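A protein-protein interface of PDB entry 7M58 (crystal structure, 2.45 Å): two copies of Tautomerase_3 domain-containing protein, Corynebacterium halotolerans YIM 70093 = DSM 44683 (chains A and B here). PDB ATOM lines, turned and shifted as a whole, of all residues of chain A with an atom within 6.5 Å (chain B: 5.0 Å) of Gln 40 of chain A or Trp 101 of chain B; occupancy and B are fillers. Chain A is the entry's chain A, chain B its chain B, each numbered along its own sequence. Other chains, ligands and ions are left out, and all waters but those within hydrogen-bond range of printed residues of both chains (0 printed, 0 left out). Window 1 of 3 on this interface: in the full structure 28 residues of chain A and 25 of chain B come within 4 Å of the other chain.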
ATOM      1  N   PRO A   1       0.364  17.459   2.913  1.00  0.00           N
ATOM      2  CA  PRO A   1      -0.605  16.501   3.461  1.00  0.00           C
ATOM      3  C   PRO A   1      -0.213  15.926   4.806  1.00  0.00           C
ATOM      4  O   PRO A   1       0.875  15.368   4.925  1.00  0.00           O
ATOM      5  CB  PRO A   1      -0.620  15.378   2.422  1.00  0.00           C
ATOM      6  CG  PRO A   1       0.748  15.427   1.820  1.00  0.00           C
ATOM      7  CD  PRO A   1       1.111  16.891   1.775  1.00  0.00           C
ATOM      8  N   SER A   2      -1.086  16.058   5.801  1.00  0.00           N
ATOM      9  CA  SER A   2      -0.883  15.442   7.108  1.00  0.00           C
ATOM     10  C   SER A   2      -2.077  14.548   7.394  1.00  0.00           C
ATOM     11  O   SER A   2      -3.216  15.018   7.427  1.00  0.00           O
ATOM     12  CB  SER A   2      -0.708  16.470   8.223  1.00  0.00           C
ATOM     13  OG  SER A   2      -1.892  17.200   8.409  1.00  0.00           O
ATOM     14  N   TYR A   3      -1.818  13.257   7.529  1.00  0.00           N
ATOM     15  CA  TYR A   3      -2.815  12.296   7.964  1.00  0.00           C
ATOM     16  C   TYR A   3      -2.757  12.144   9.478  1.00  0.00           C
ATOM     17  O   TYR A   3      -1.708  11.789  10.028  1.00  0.00           O
ATOM     18  CB  TYR A   3      -2.585  10.950   7.283  1.00  0.00           C
ATOM     19  CG  TYR A   3      -2.836  11.006   5.803  1.00  0.00           C
ATOM     20  CD1 TYR A   3      -1.843  11.417   4.926  1.00  0.00           C
ATOM     21  CD2 TYR A   3      -4.078  10.665   5.281  1.00  0.00           C
ATOM     22  CE1 TYR A   3      -2.068  11.477   3.576  1.00  0.00           C
ATOM     23  CE2 TYR A   3      -4.309  10.721   3.926  1.00  0.00           C
ATOM     24  CZ  TYR A   3      -3.302  11.137   3.080  1.00  0.00           C
ATOM     25  OH  TYR A   3      -3.522  11.192   1.725  1.00  0.00           O
ATOM     26  N   ALA A   4      -3.870  12.418  10.150  1.00  0.00           N
ATOM     27  CA  ALA A   4      -4.005  12.103  11.563  1.00  0.00           C
ATOM     28  C   ALA A   4      -4.878  10.861  11.689  1.00  0.00           C
ATOM     29  O   ALA A   4      -5.948  10.778  11.080  1.00  0.00           O
ATOM     30  CB  ALA A   4      -4.584  13.281  12.339  1.00  0.00           C
ATOM     31  N   THR A  25       1.537   7.146   2.865  1.00  0.00           N
ATOM     32  CA  THR A  25       2.496   7.945   2.110  1.00  0.00           C
ATOM     33  C   THR A  25       2.612   7.446   0.669  1.00  0.00           C
ATOM     34  O   THR A  25       2.839   8.238  -0.257  1.00  0.00           O
ATOM     35  CB  THR A  25       3.857   7.905   2.818  1.00  0.00           C
ATOM     36  OG1 THR A  25       3.755   8.513   4.115  1.00  0.00           O
ATOM     37  CG2 THR A  25       4.916   8.602   2.011  1.00  0.00           C
ATOM     38  N   ARG A  36       6.597  12.143  -1.809  1.00  0.00           N
ATOM     39  CA  ARG A  36       6.452  11.567  -0.476  1.00  0.00           C
ATOM     40  C   ARG A  36       6.970  12.508   0.606  1.00  0.00           C
ATOM     41  O   ARG A  36       6.473  12.475   1.748  1.00  0.00           O
ATOM     42  CB  ARG A  36       7.175  10.223  -0.391  1.00  0.00           C
ATOM     43  CG  ARG A  36       6.985   9.350  -1.590  1.00  0.00           C
ATOM     44  CD  ARG A  36       7.388   7.889  -1.237  1.00  0.00           C
ATOM     45  NE  ARG A  36       6.267   7.109  -0.730  1.00  0.00           N
ATOM     46  CZ  ARG A  36       6.064   5.834  -1.048  1.00  0.00           C
ATOM     47  NH1 ARG A  36       6.949   5.271  -1.842  1.00  0.00           N
ATOM     48  NH2 ARG A  36       4.983   5.144  -0.622  1.00  0.00           N
ATOM     49  N   TYR A  37       7.997  13.319   0.293  1.00  0.00           N
ATOM     50  CA  TYR A  37       8.594  14.112   1.361  1.00  0.00           C
ATOM     51  C   TYR A  37       7.616  15.143   1.921  1.00  0.00           C
ATOM     52  O   TYR A  37       7.906  15.748   2.959  1.00  0.00           O
ATOM     53  CB  TYR A  37       9.892  14.818   0.891  1.00  0.00           C
ATOM     54  CG  TYR A  37       9.777  15.732  -0.323  1.00  0.00           C
ATOM     55  CD1 TYR A  37       9.058  16.924  -0.246  1.00  0.00           C
ATOM     56  CD2 TYR A  37      10.410  15.428  -1.539  1.00  0.00           C
ATOM     57  CE1 TYR A  37       8.932  17.774  -1.336  1.00  0.00           C
ATOM     58  CE2 TYR A  37      10.290  16.281  -2.642  1.00  0.00           C
ATOM     59  CZ  TYR A  37       9.545  17.455  -2.524  1.00  0.00           C
ATOM     60  OH  TYR A  37       9.375  18.327  -3.572  1.00  0.00           O
ATOM     61  N   LEU A  38       6.460  15.336   1.283  1.00  0.00           N
ATOM     62  CA  LEU A  38       5.465  16.255   1.807  1.00  0.00           C
ATOM     63  C   LEU A  38       4.552  15.612   2.840  1.00  0.00           C
ATOM     64  O   LEU A  38       3.815  16.327   3.526  1.00  0.00           O
ATOM     65  CB  LEU A  38       4.607  16.816   0.668  1.00  0.00           C
ATOM     66  CG  LEU A  38       5.246  17.830  -0.294  1.00  0.00           C
ATOM     67  CD1 LEU A  38       4.174  18.531  -1.129  1.00  0.00           C
ATOM     68  CD2 LEU A  38       6.105  18.831   0.433  1.00  0.00           C
ATOM     69  N   VAL A  39       4.590  14.294   2.975  1.00  0.00           N
ATOM     70  CA  VAL A  39       3.563  13.568   3.705  1.00  0.00           C
ATOM     71  C   VAL A  39       3.966  13.418   5.169  1.00  0.00           C
ATOM     72  O   VAL A  39       5.059  12.929   5.494  1.00  0.00           O
ATOM     73  CB  VAL A  39       3.304  12.197   3.063  1.00  0.00           C
ATOM     74  CG1 VAL A  39       2.159  11.502   3.778  1.00  0.00           C
ATOM     75  CG2 VAL A  39       3.055  12.344   1.564  1.00  0.00           C
ATOM     76  N   GLN A  40       3.068  13.829   6.052  1.00  0.00           N
ATOM     77  CA  GLN A  40       3.197  13.652   7.482  1.00  0.00           C
ATOM     78  C   GLN A  40       2.071  12.742   7.962  1.00  0.00           C
ATOM     79  O   GLN A  40       0.927  12.891   7.529  1.00  0.00           O
ATOM     80  CB  GLN A  40       3.146  15.019   8.180  1.00  0.00           C
ATOM     81  CG  GLN A  40       3.015  14.975   9.681  1.00  0.00           C
ATOM     82  CD  GLN A  40       2.933  16.368  10.275  1.00  0.00           C
ATOM     83  OE1 GLN A  40       3.941  16.942  10.696  1.00  0.00           O
ATOM     84  NE2 GLN A  40       1.729  16.920  10.316  1.00  0.00           N
ATOM     85  N   VAL A  41       2.397  11.783   8.828  1.00  0.00           N
ATOM     86  CA  VAL A  41       1.407  10.901   9.435  1.00  0.00           C
ATOM     87  C   VAL A  41       1.531  11.007  10.945  1.00  0.00           C
ATOM     88  O   VAL A  41       2.631  10.874  11.497  1.00  0.00           O
ATOM     89  CB  VAL A  41       1.576   9.434   9.005  1.00  0.00           C
ATOM     90  CG1 VAL A  41       0.562   8.565   9.753  1.00  0.00           C
ATOM     91  CG2 VAL A  41       1.409   9.279   7.507  1.00  0.00           C
ATOM     92  N   ILE A  42       0.410  11.215  11.615  1.00  0.00           N
ATOM     93  CA  ILE A  42       0.402  11.342  13.063  1.00  0.00           C
ATOM     94  C   ILE A  42      -0.598  10.344  13.628  1.00  0.00           C
ATOM     95  O   ILE A  42      -1.702  10.190  13.093  1.00  0.00           O
ATOM     96  CB  ILE A  42       0.067  12.777  13.494  1.00  0.00           C
ATOM     97  CG1 ILE A  42       1.237  13.687  13.178  1.00  0.00           C
ATOM     98  CG2 ILE A  42      -0.180  12.821  14.958  1.00  0.00           C
ATOM     99  CD1 ILE A  42       0.820  15.136  13.010  1.00  0.00           C
ATOM    100  N   THR A 113       2.739  25.844   5.433  1.00  0.00           N
ATOM    101  CA  THR A 113       4.191  25.804   5.330  1.00  0.00           C
ATOM    102  C   THR A 113       4.629  24.381   5.636  1.00  0.00           C
ATOM    103  O   THR A 113       4.099  23.736   6.542  1.00  0.00           O
ATOM    104  CB  THR A 113       4.922  26.784   6.271  1.00  0.00           C
ATOM    105  OG1 THR A 113       4.682  26.437   7.645  1.00  0.00           O
ATOM    106  CG2 THR A 113       4.511  28.211   6.018  1.00  0.00           C
ATOM    107  N   GLU A 114       5.576  23.898   4.849  1.00  0.00           N
ATOM    108  CA  GLU A 114       6.298  22.663   5.091  1.00  0.00           C
ATOM    109  C   GLU A 114       7.717  22.912   4.604  1.00  0.00           C
ATOM    110  O   GLU A 114       7.916  23.561   3.571  1.00  0.00           O
ATOM    111  CB  GLU A 114       5.669  21.478   4.343  1.00  0.00           C
ATOM    112  CG  GLU A 114       4.282  21.079   4.813  1.00  0.00           C
ATOM    113  CD  GLU A 114       3.782  19.806   4.120  1.00  0.00           C
ATOM    114  OE1 GLU A 114       4.614  19.125   3.462  1.00  0.00           O
ATOM    115  OE2 GLU A 114       2.570  19.468   4.242  1.00  0.00           O
ATOM    116  N   TYR A 115       8.701  22.428   5.367  1.00  0.00           N
ATOM    117  CA  TYR A 115      10.113  22.711   5.098  1.00  0.00           C
ATOM    118  C   TYR A 115      10.396  24.211   5.053  1.00  0.00           C
ATOM    119  O   TYR A 115      11.236  24.675   4.284  1.00  0.00           O
ATOM    120  CB  TYR A 115      10.573  22.023   3.811  1.00  0.00           C
ATOM    121  CG  TYR A 115      10.352  20.543   3.907  1.00  0.00           C
ATOM    122  CD1 TYR A 115      11.160  19.753   4.726  1.00  0.00           C
ATOM    123  CD2 TYR A 115       9.328  19.931   3.213  1.00  0.00           C
ATOM    124  CE1 TYR A 115      10.960  18.396   4.842  1.00  0.00           C
ATOM    125  CE2 TYR A 115       9.124  18.569   3.314  1.00  0.00           C
ATOM    126  CZ  TYR A 115       9.943  17.811   4.132  1.00  0.00           C
ATOM    127  OH  TYR A 115       9.740  16.468   4.241  1.00  0.00           O
ATOM    128  N   GLY A 116       9.687  24.975   5.878  1.00  0.00           N
ATOM    129  CA  GLY A 116       9.915  26.400   6.005  1.00  0.00           C
ATOM    130  C   GLY A 116       9.396  27.270   4.874  1.00  0.00           C
ATOM    131  O   GLY A 116       9.701  28.470   4.851  1.00  0.00           O
ATOM    132  N   LEU B  51       4.964   9.847  15.075  1.00  0.00           N
ATOM    133  CA  LEU B  51       5.042  10.879  14.055  1.00  0.00           C
ATOM    134  C   LEU B  51       5.917  10.373  12.914  1.00  0.00           C
ATOM    135  O   LEU B  51       7.036   9.914  13.142  1.00  0.00           O
ATOM    136  CB  LEU B  51       5.577  12.178  14.659  1.00  0.00           C
ATOM    137  CG  LEU B  51       5.044  13.471  14.032  1.00  0.00           C
ATOM    138  CD1 LEU B  51       5.296  14.633  14.988  1.00  0.00           C
ATOM    139  CD2 LEU B  51       5.580  13.762  12.632  1.00  0.00           C
ATOM    140  N   PHE B  52       5.399  10.421  11.699  1.00  0.00           N
ATOM    141  CA  PHE B  52       6.114   9.960  10.518  1.00  0.00           C
ATOM    142  C   PHE B  52       6.173  11.078   9.488  1.00  0.00           C
ATOM    143  O   PHE B  52       5.222  11.854   9.342  1.00  0.00           O
ATOM    144  CB  PHE B  52       5.446   8.727   9.899  1.00  0.00           C
ATOM    145  CG  PHE B  52       5.525   7.494  10.749  1.00  0.00           C
ATOM    146  CD1 PHE B  52       4.723   7.357  11.872  1.00  0.00           C
ATOM    147  CD2 PHE B  52       6.378   6.452  10.404  1.00  0.00           C
ATOM    148  CE1 PHE B  52       4.789   6.220  12.658  1.00  0.00           C
ATOM    149  CE2 PHE B  52       6.443   5.291  11.189  1.00  0.00           C
ATOM    150  CZ  PHE B  52       5.645   5.178  12.314  1.00  0.00           C
ATOM    151  N   LEU B  53       7.310  11.169   8.805  1.00  0.00           N
ATOM    152  CA  LEU B  53       7.543  12.099   7.711  1.00  0.00           C
ATOM    153  C   LEU B  53       8.091  11.333   6.515  1.00  0.00           C
ATOM    154  O   LEU B  53       9.072  10.602   6.651  1.00  0.00           O
ATOM    155  CB  LEU B  53       8.532  13.199   8.128  1.00  0.00           C
ATOM    156  CG  LEU B  53       7.961  14.209   9.107  1.00  0.00           C
ATOM    157  CD1 LEU B  53       9.072  15.064   9.710  1.00  0.00           C
ATOM    158  CD2 LEU B  53       6.866  15.049   8.448  1.00  0.00           C
ATOM    159  N   HIS B  62      10.498  18.037  15.587  1.00  0.00           N
ATOM    160  CA  HIS B  62       9.491  18.383  14.599  1.00  0.00           C
ATOM    161  C   HIS B  62       8.206  18.775  15.317  1.00  0.00           C
ATOM    162  O   HIS B  62       7.783  18.093  16.256  1.00  0.00           O
ATOM    163  CB  HIS B  62       9.286  17.209  13.635  1.00  0.00           C
ATOM    164  CG  HIS B  62       8.323  17.486  12.538  1.00  0.00           C
ATOM    165  ND1 HIS B  62       8.679  18.168  11.393  1.00  0.00           N
ATOM    166  CD2 HIS B  62       7.026  17.136  12.383  1.00  0.00           C
ATOM    167  CE1 HIS B  62       7.628  18.263  10.597  1.00  0.00           C
ATOM    168  NE2 HIS B  62       6.615  17.636  11.171  1.00  0.00           N
ATOM    169  N   VAL B  63       7.597  19.873  14.873  1.00  0.00           N
ATOM    170  CA  VAL B  63       6.373  20.416  15.445  1.00  0.00           C
ATOM    171  C   VAL B  63       5.401  20.706  14.307  1.00  0.00           C
ATOM    172  O   VAL B  63       5.789  21.262  13.272  1.00  0.00           O
ATOM    173  CB  VAL B  63       6.661  21.701  16.256  1.00  0.00           C
ATOM    174  CG1 VAL B  63       5.369  22.442  16.591  1.00  0.00           C
ATOM    175  CG2 VAL B  63       7.393  21.364  17.533  1.00  0.00           C
ATOM    176  N   TRP B  64       4.136  20.321  14.492  1.00  0.00           N
ATOM    177  CA  TRP B  64       3.076  20.639  13.540  1.00  0.00           C
ATOM    178  C   TRP B  64       2.015  21.471  14.241  1.00  0.00           C
ATOM    179  O   TRP B  64       1.471  21.052  15.269  1.00  0.00           O
ATOM    180  CB  TRP B  64       2.446  19.380  12.947  1.00  0.00           C
ATOM    181  CG  TRP B  64       1.331  19.662  11.994  1.00  0.00           C
ATOM    182  CD1 TRP B  64       1.374  20.445  10.860  1.00  0.00           C
ATOM    183  CD2 TRP B  64      -0.017  19.202  12.107  1.00  0.00           C
ATOM    184  NE1 TRP B  64       0.141  20.469  10.252  1.00  0.00           N
ATOM    185  CE2 TRP B  64      -0.734  19.721  11.003  1.00  0.00           C
ATOM    186  CE3 TRP B  64      -0.689  18.388  13.030  1.00  0.00           C
ATOM    187  CZ2 TRP B  64      -2.094  19.459  10.805  1.00  0.00           C
ATOM    188  CZ3 TRP B  64      -2.027  18.124  12.826  1.00  0.00           C
ATOM    189  CH2 TRP B  64      -2.722  18.661  11.722  1.00  0.00           C
ATOM    190  N   ILE B  65       1.708  22.631  13.666  1.00  0.00           N
ATOM    191  CA  ILE B  65       0.756  23.579  14.229  1.00  0.00           C
ATOM    192  C   ILE B  65      -0.471  23.631  13.323  1.00  0.00           C
ATOM    193  O   ILE B  65      -0.343  23.878  12.117  1.00  0.00           O
ATOM    194  CB  ILE B  65       1.388  24.966  14.400  1.00  0.00           C
ATOM    195  CG1 ILE B  65       2.648  24.874  15.302  1.00  0.00           C
ATOM    196  CG2 ILE B  65       0.347  25.938  14.926  1.00  0.00           C
ATOM    197  CD1 ILE B  65       3.535  26.157  15.338  1.00  0.00           C
ATOM    198  N   GLU B  98      12.390  24.524   8.945  1.00  0.00           N
ATOM    199  CA  GLU B  98      11.931  23.437   8.110  1.00  0.00           C
ATOM    200  C   GLU B  98      11.175  22.392   8.896  1.00  0.00           C
ATOM    201  O   GLU B  98      10.608  21.479   8.291  1.00  0.00           O
ATOM    202  CB  GLU B  98      13.124  22.774   7.423  1.00  0.00           C
ATOM    203  CG  GLU B  98      13.832  23.648   6.408  1.00  0.00           C
ATOM    204  CD  GLU B  98      14.746  24.680   7.061  1.00  0.00           C
ATOM    205  OE1 GLU B  98      15.078  24.535   8.259  1.00  0.00           O
ATOM    206  OE2 GLU B  98      15.114  25.664   6.381  1.00  0.00           O
ATOM    207  N   HIS B  99      11.198  22.461  10.225  1.00  0.00           N
ATOM    208  CA  HIS B  99      10.550  21.448  11.047  1.00  0.00           C
ATOM    209  C   HIS B  99       9.505  22.046  11.981  1.00  0.00           C
ATOM    210  O   HIS B  99       9.108  21.412  12.970  1.00  0.00           O
ATOM    211  CB  HIS B  99      11.618  20.627  11.773  1.00  0.00           C
ATOM    212  CG  HIS B  99      12.181  19.552  10.901  1.00  0.00           C
ATOM    213  ND1 HIS B  99      11.382  18.588  10.318  1.00  0.00           N
ATOM    214  CD2 HIS B  99      13.419  19.381  10.378  1.00  0.00           C
ATOM    215  CE1 HIS B  99      12.122  17.820   9.538  1.00  0.00           C
ATOM    216  NE2 HIS B  99      13.361  18.279   9.559  1.00  0.00           N
ATOM    217  N   VAL B 100       9.041  23.248  11.666  1.00  0.00           N
ATOM    218  CA  VAL B 100       7.806  23.790  12.205  1.00  0.00           C
ATOM    219  C   VAL B 100       6.864  23.923  11.016  1.00  0.00           C
ATOM    220  O   VAL B 100       6.964  24.878  10.240  1.00  0.00           O
ATOM    221  CB  VAL B 100       8.030  25.133  12.912  1.00  0.00           C
ATOM    222  CG1 VAL B 100       6.721  25.683  13.447  1.00  0.00           C
ATOM    223  CG2 VAL B 100       9.048  24.975  14.045  1.00  0.00           C
ATOM    224  N   TRP B 101       5.950  22.971  10.857  1.00  0.00           N
ATOM    225  CA  TRP B 101       4.991  22.986   9.755  1.00  0.00           C
ATOM    226  C   TRP B 101       3.684  23.570  10.269  1.00  0.00           C
ATOM    227  O   TRP B 101       3.215  23.178  11.345  1.00  0.00           O
ATOM    228  CB  TRP B 101       4.740  21.588   9.219  1.00  0.00           C
ATOM    229  CG  TRP B 101       5.909  20.948   8.579  1.00  0.00           C
ATOM    230  CD1 TRP B 101       7.215  21.301   8.708  1.00  0.00           C
ATOM    231  CD2 TRP B 101       5.886  19.780   7.747  1.00  0.00           C
ATOM    232  NE1 TRP B 101       8.014  20.438   7.990  1.00  0.00           N
ATOM    233  CE2 TRP B 101       7.223  19.496   7.390  1.00  0.00           C
ATOM    234  CE3 TRP B 101       4.860  18.948   7.262  1.00  0.00           C
ATOM    235  CZ2 TRP B 101       7.565  18.416   6.572  1.00  0.00           C
ATOM    236  CZ3 TRP B 101       5.197  17.878   6.446  1.00  0.00           C
ATOM    237  CH2 TRP B 101       6.539  17.622   6.109  1.00  0.00           C
ATOM    238  N   VAL B 102       3.106  24.514   9.515  1.00  0.00           N
ATOM    239  CA  VAL B 102       1.923  25.258   9.945  1.00  0.00           C
ATOM    240  C   VAL B 102       0.821  25.146   8.902  1.00  0.00           C
ATOM    241  O   VAL B 102       1.052  25.416   7.718  1.00  0.00           O
ATOM    242  CB  VAL B 102       2.237  26.743  10.198  1.00  0.00           C
ATOM    243  CG1 VAL B 102       1.071  27.399  10.916  1.00  0.00           C
ATOM    244  CG2 VAL B 102       3.530  26.904  10.992  1.00  0.00           C
ATOM    245  N   TYR B 103      -0.380  24.770   9.350  1.00  0.00           N
ATOM    246  CA  TYR B 103      -1.595  24.739   8.548  1.00  0.00           C
ATOM    247  C   TYR B 103      -2.619  25.659   9.195  1.00  0.00           C
ATOM    248  O   TYR B 103      -2.824  25.596  10.415  1.00  0.00           O
ATOM    249  CB  TYR B 103      -2.206  23.333   8.497  1.00  0.00           C
ATOM    250  CG  TYR B 103      -1.481  22.300   7.671  1.00  0.00           C
ATOM    251  CD1 TYR B 103      -0.173  22.491   7.256  1.00  0.00           C
ATOM    252  CD2 TYR B 103      -2.125  21.130   7.293  1.00  0.00           C
ATOM    253  CE1 TYR B 103       0.482  21.534   6.508  1.00  0.00           C
ATOM    254  CE2 TYR B 103      -1.484  20.173   6.533  1.00  0.00           C
ATOM    255  CZ  TYR B 103      -0.177  20.376   6.149  1.00  0.00           C
ATOM    256  OH  TYR B 103       0.469  19.429   5.398  1.00  0.00           O
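Along chain A the printed residues that touch a printed residue of chain B span positions 1 to 116.
Hydrophobic or aromatic side chains of chain B within 4 Å of the printed part of chain A: Leu 51, Phe 52, Leu 53, His 62, Trp 64, Trp 101, Val 102 and Tyr 103.
Among the printed residues, 24 pairs touch across the chains.
Among the printed residues, merely in contact across the chains: Ser 2 of chain A with Trp 64 of chain B (3.3 Å), Ser 2 of chain A with Tyr 103 of chain B (3.5 Å), Tyr 37 of chain A with Trp 101 of chain B (3.9 Å), Leu 38 of chain A with Trp 101 of chain B (3.6 Å), Val 39 of chain A with Phe 52 of chain B (3.999 Å), Val 39 of chain A with Leu 53 of chain B (3.4 Å), Gln 40 of chain A with Phe 52 of chain B (3.3 Å), Gln 40 of chain A with Leu 53 of chain B (3.7 Å), Gln 40 of chain A with Trp 64 of chain B (3.2 Å), Gln 40 of chain A with Trp 101 of chain B (3.9 Å), Val 41 of chain A with Leu 51 of chain B (3.5 Å), Ile 42 of chain A with Leu 51 of chain B (3.9 Å), Ile 42 of chain A with Trp 64 of chain B (3.6 Å), Thr 113 of chain A with Val 100 of chain B (3.8 Å), Thr 113 of chain A with Trp 101 of chain B (3.4 Å), Glu 114 of chain A with Trp 101 of chain B (3.3 Å), Tyr 115 of chain A with Glu 98 of chain B (3.5 Å) and Gly 116 of chain A with Glu 98 of chain B (3.5 Å).
No position is printed for both chains.
Of the 24 pairs that touch across the chains among the printed residues, none has its exchanged pair printed and touching as well.
OE1 of Gln 40 of chain A sits at hydrogen-bond distance from NE2 of His 62 of chain B (2.8 Å).
The backbone carbonyl oxygen of Val 41 of chain A sits at hydrogen-bond distance from the backbone NH of Phe 52 of chain B (2.8 Å).
O of Val 102 of chain B lies within hydrogen-bond range of N of Thr 113 of chain A, at 2.9 Å.
N of Pro 1 of chain A sits close to OH of Tyr 103 of chain B, at 3.2 Å.
The side-chain carboxylate (OE2) of Glu 114 of chain A sits close to the side-chain hydroxyl (OH) of Tyr 103 of chain B (2.4 Å).
The indole nitrogen of Trp 101 of chain B sits close to the backbone NH of Tyr 115 of chain A (3.4 Å).
O of Pro 1 of chain A lies within hydrogen-bond range of N of Gln 40 of chain A, 2.9 Å away.
The backbone carbonyl oxygen of Gln 40 of chain A is in hydrogen-bond range of the backbone NH of Tyr 3 of chain A.
The backbone NH (N) of Ile 42 of chain A is in hydrogen-bond range of the backbone carbonyl oxygen (O) of Tyr 3 of chain A (2.7 Å).
ND1 of His 62 of chain B sits at hydrogen-bond distance from ND1 of His 99 of chain B.
The backbone NH (N) of Tyr 103 of chain B sits at hydrogen-bond distance from the backbone carbonyl oxygen (O) of Ile 65 of chain B (2.9 Å).
O of Glu 98 of chain B lies within hydrogen-bond range of NE1 of Trp 101 of chain B (2.8 Å).
Gln 40 of chain A touches just these residues of chain B: Phe 52 (3.3 Å), Leu 53 (3.7 Å), His 62 (2.8 Å), Trp 64 (3.2 Å) and Trp 101 (3.9 Å).
Trp 101 of chain B touches just these residues of chain A: Tyr 37 (3.9 Å), Leu 38 (3.6 Å), Gln 40 (3.9 Å), Thr 113 (3.4 Å), Glu 114 (3.3 Å) and Tyr 115 (3.4 Å).
Printed residues of chain A within 4 Å of Leu 53 of chain B: Val 39 (3.4 Å) and Gln 40 (3.7 Å).
Of the printed residues of chain B, Thr 113 of chain A touches Val 100, Trp 101 and Val 102.
Of the printed residues of chain B, Val 39 of chain A touches Phe 52 (3.999 Å) and Leu 53 (3.4 Å).
Printed residues of chain B within 4 Å of Tyr 37 of chain A: Trp 101.
Ala 4 of chain A touches none of the printed residues of chain B.
Arg 36 of chain A touches none of the printed residues of chain B.
The nearest residue of chain B that does not touch Gln 40 of chain A is Leu 51 of chain B (4.1 Å).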
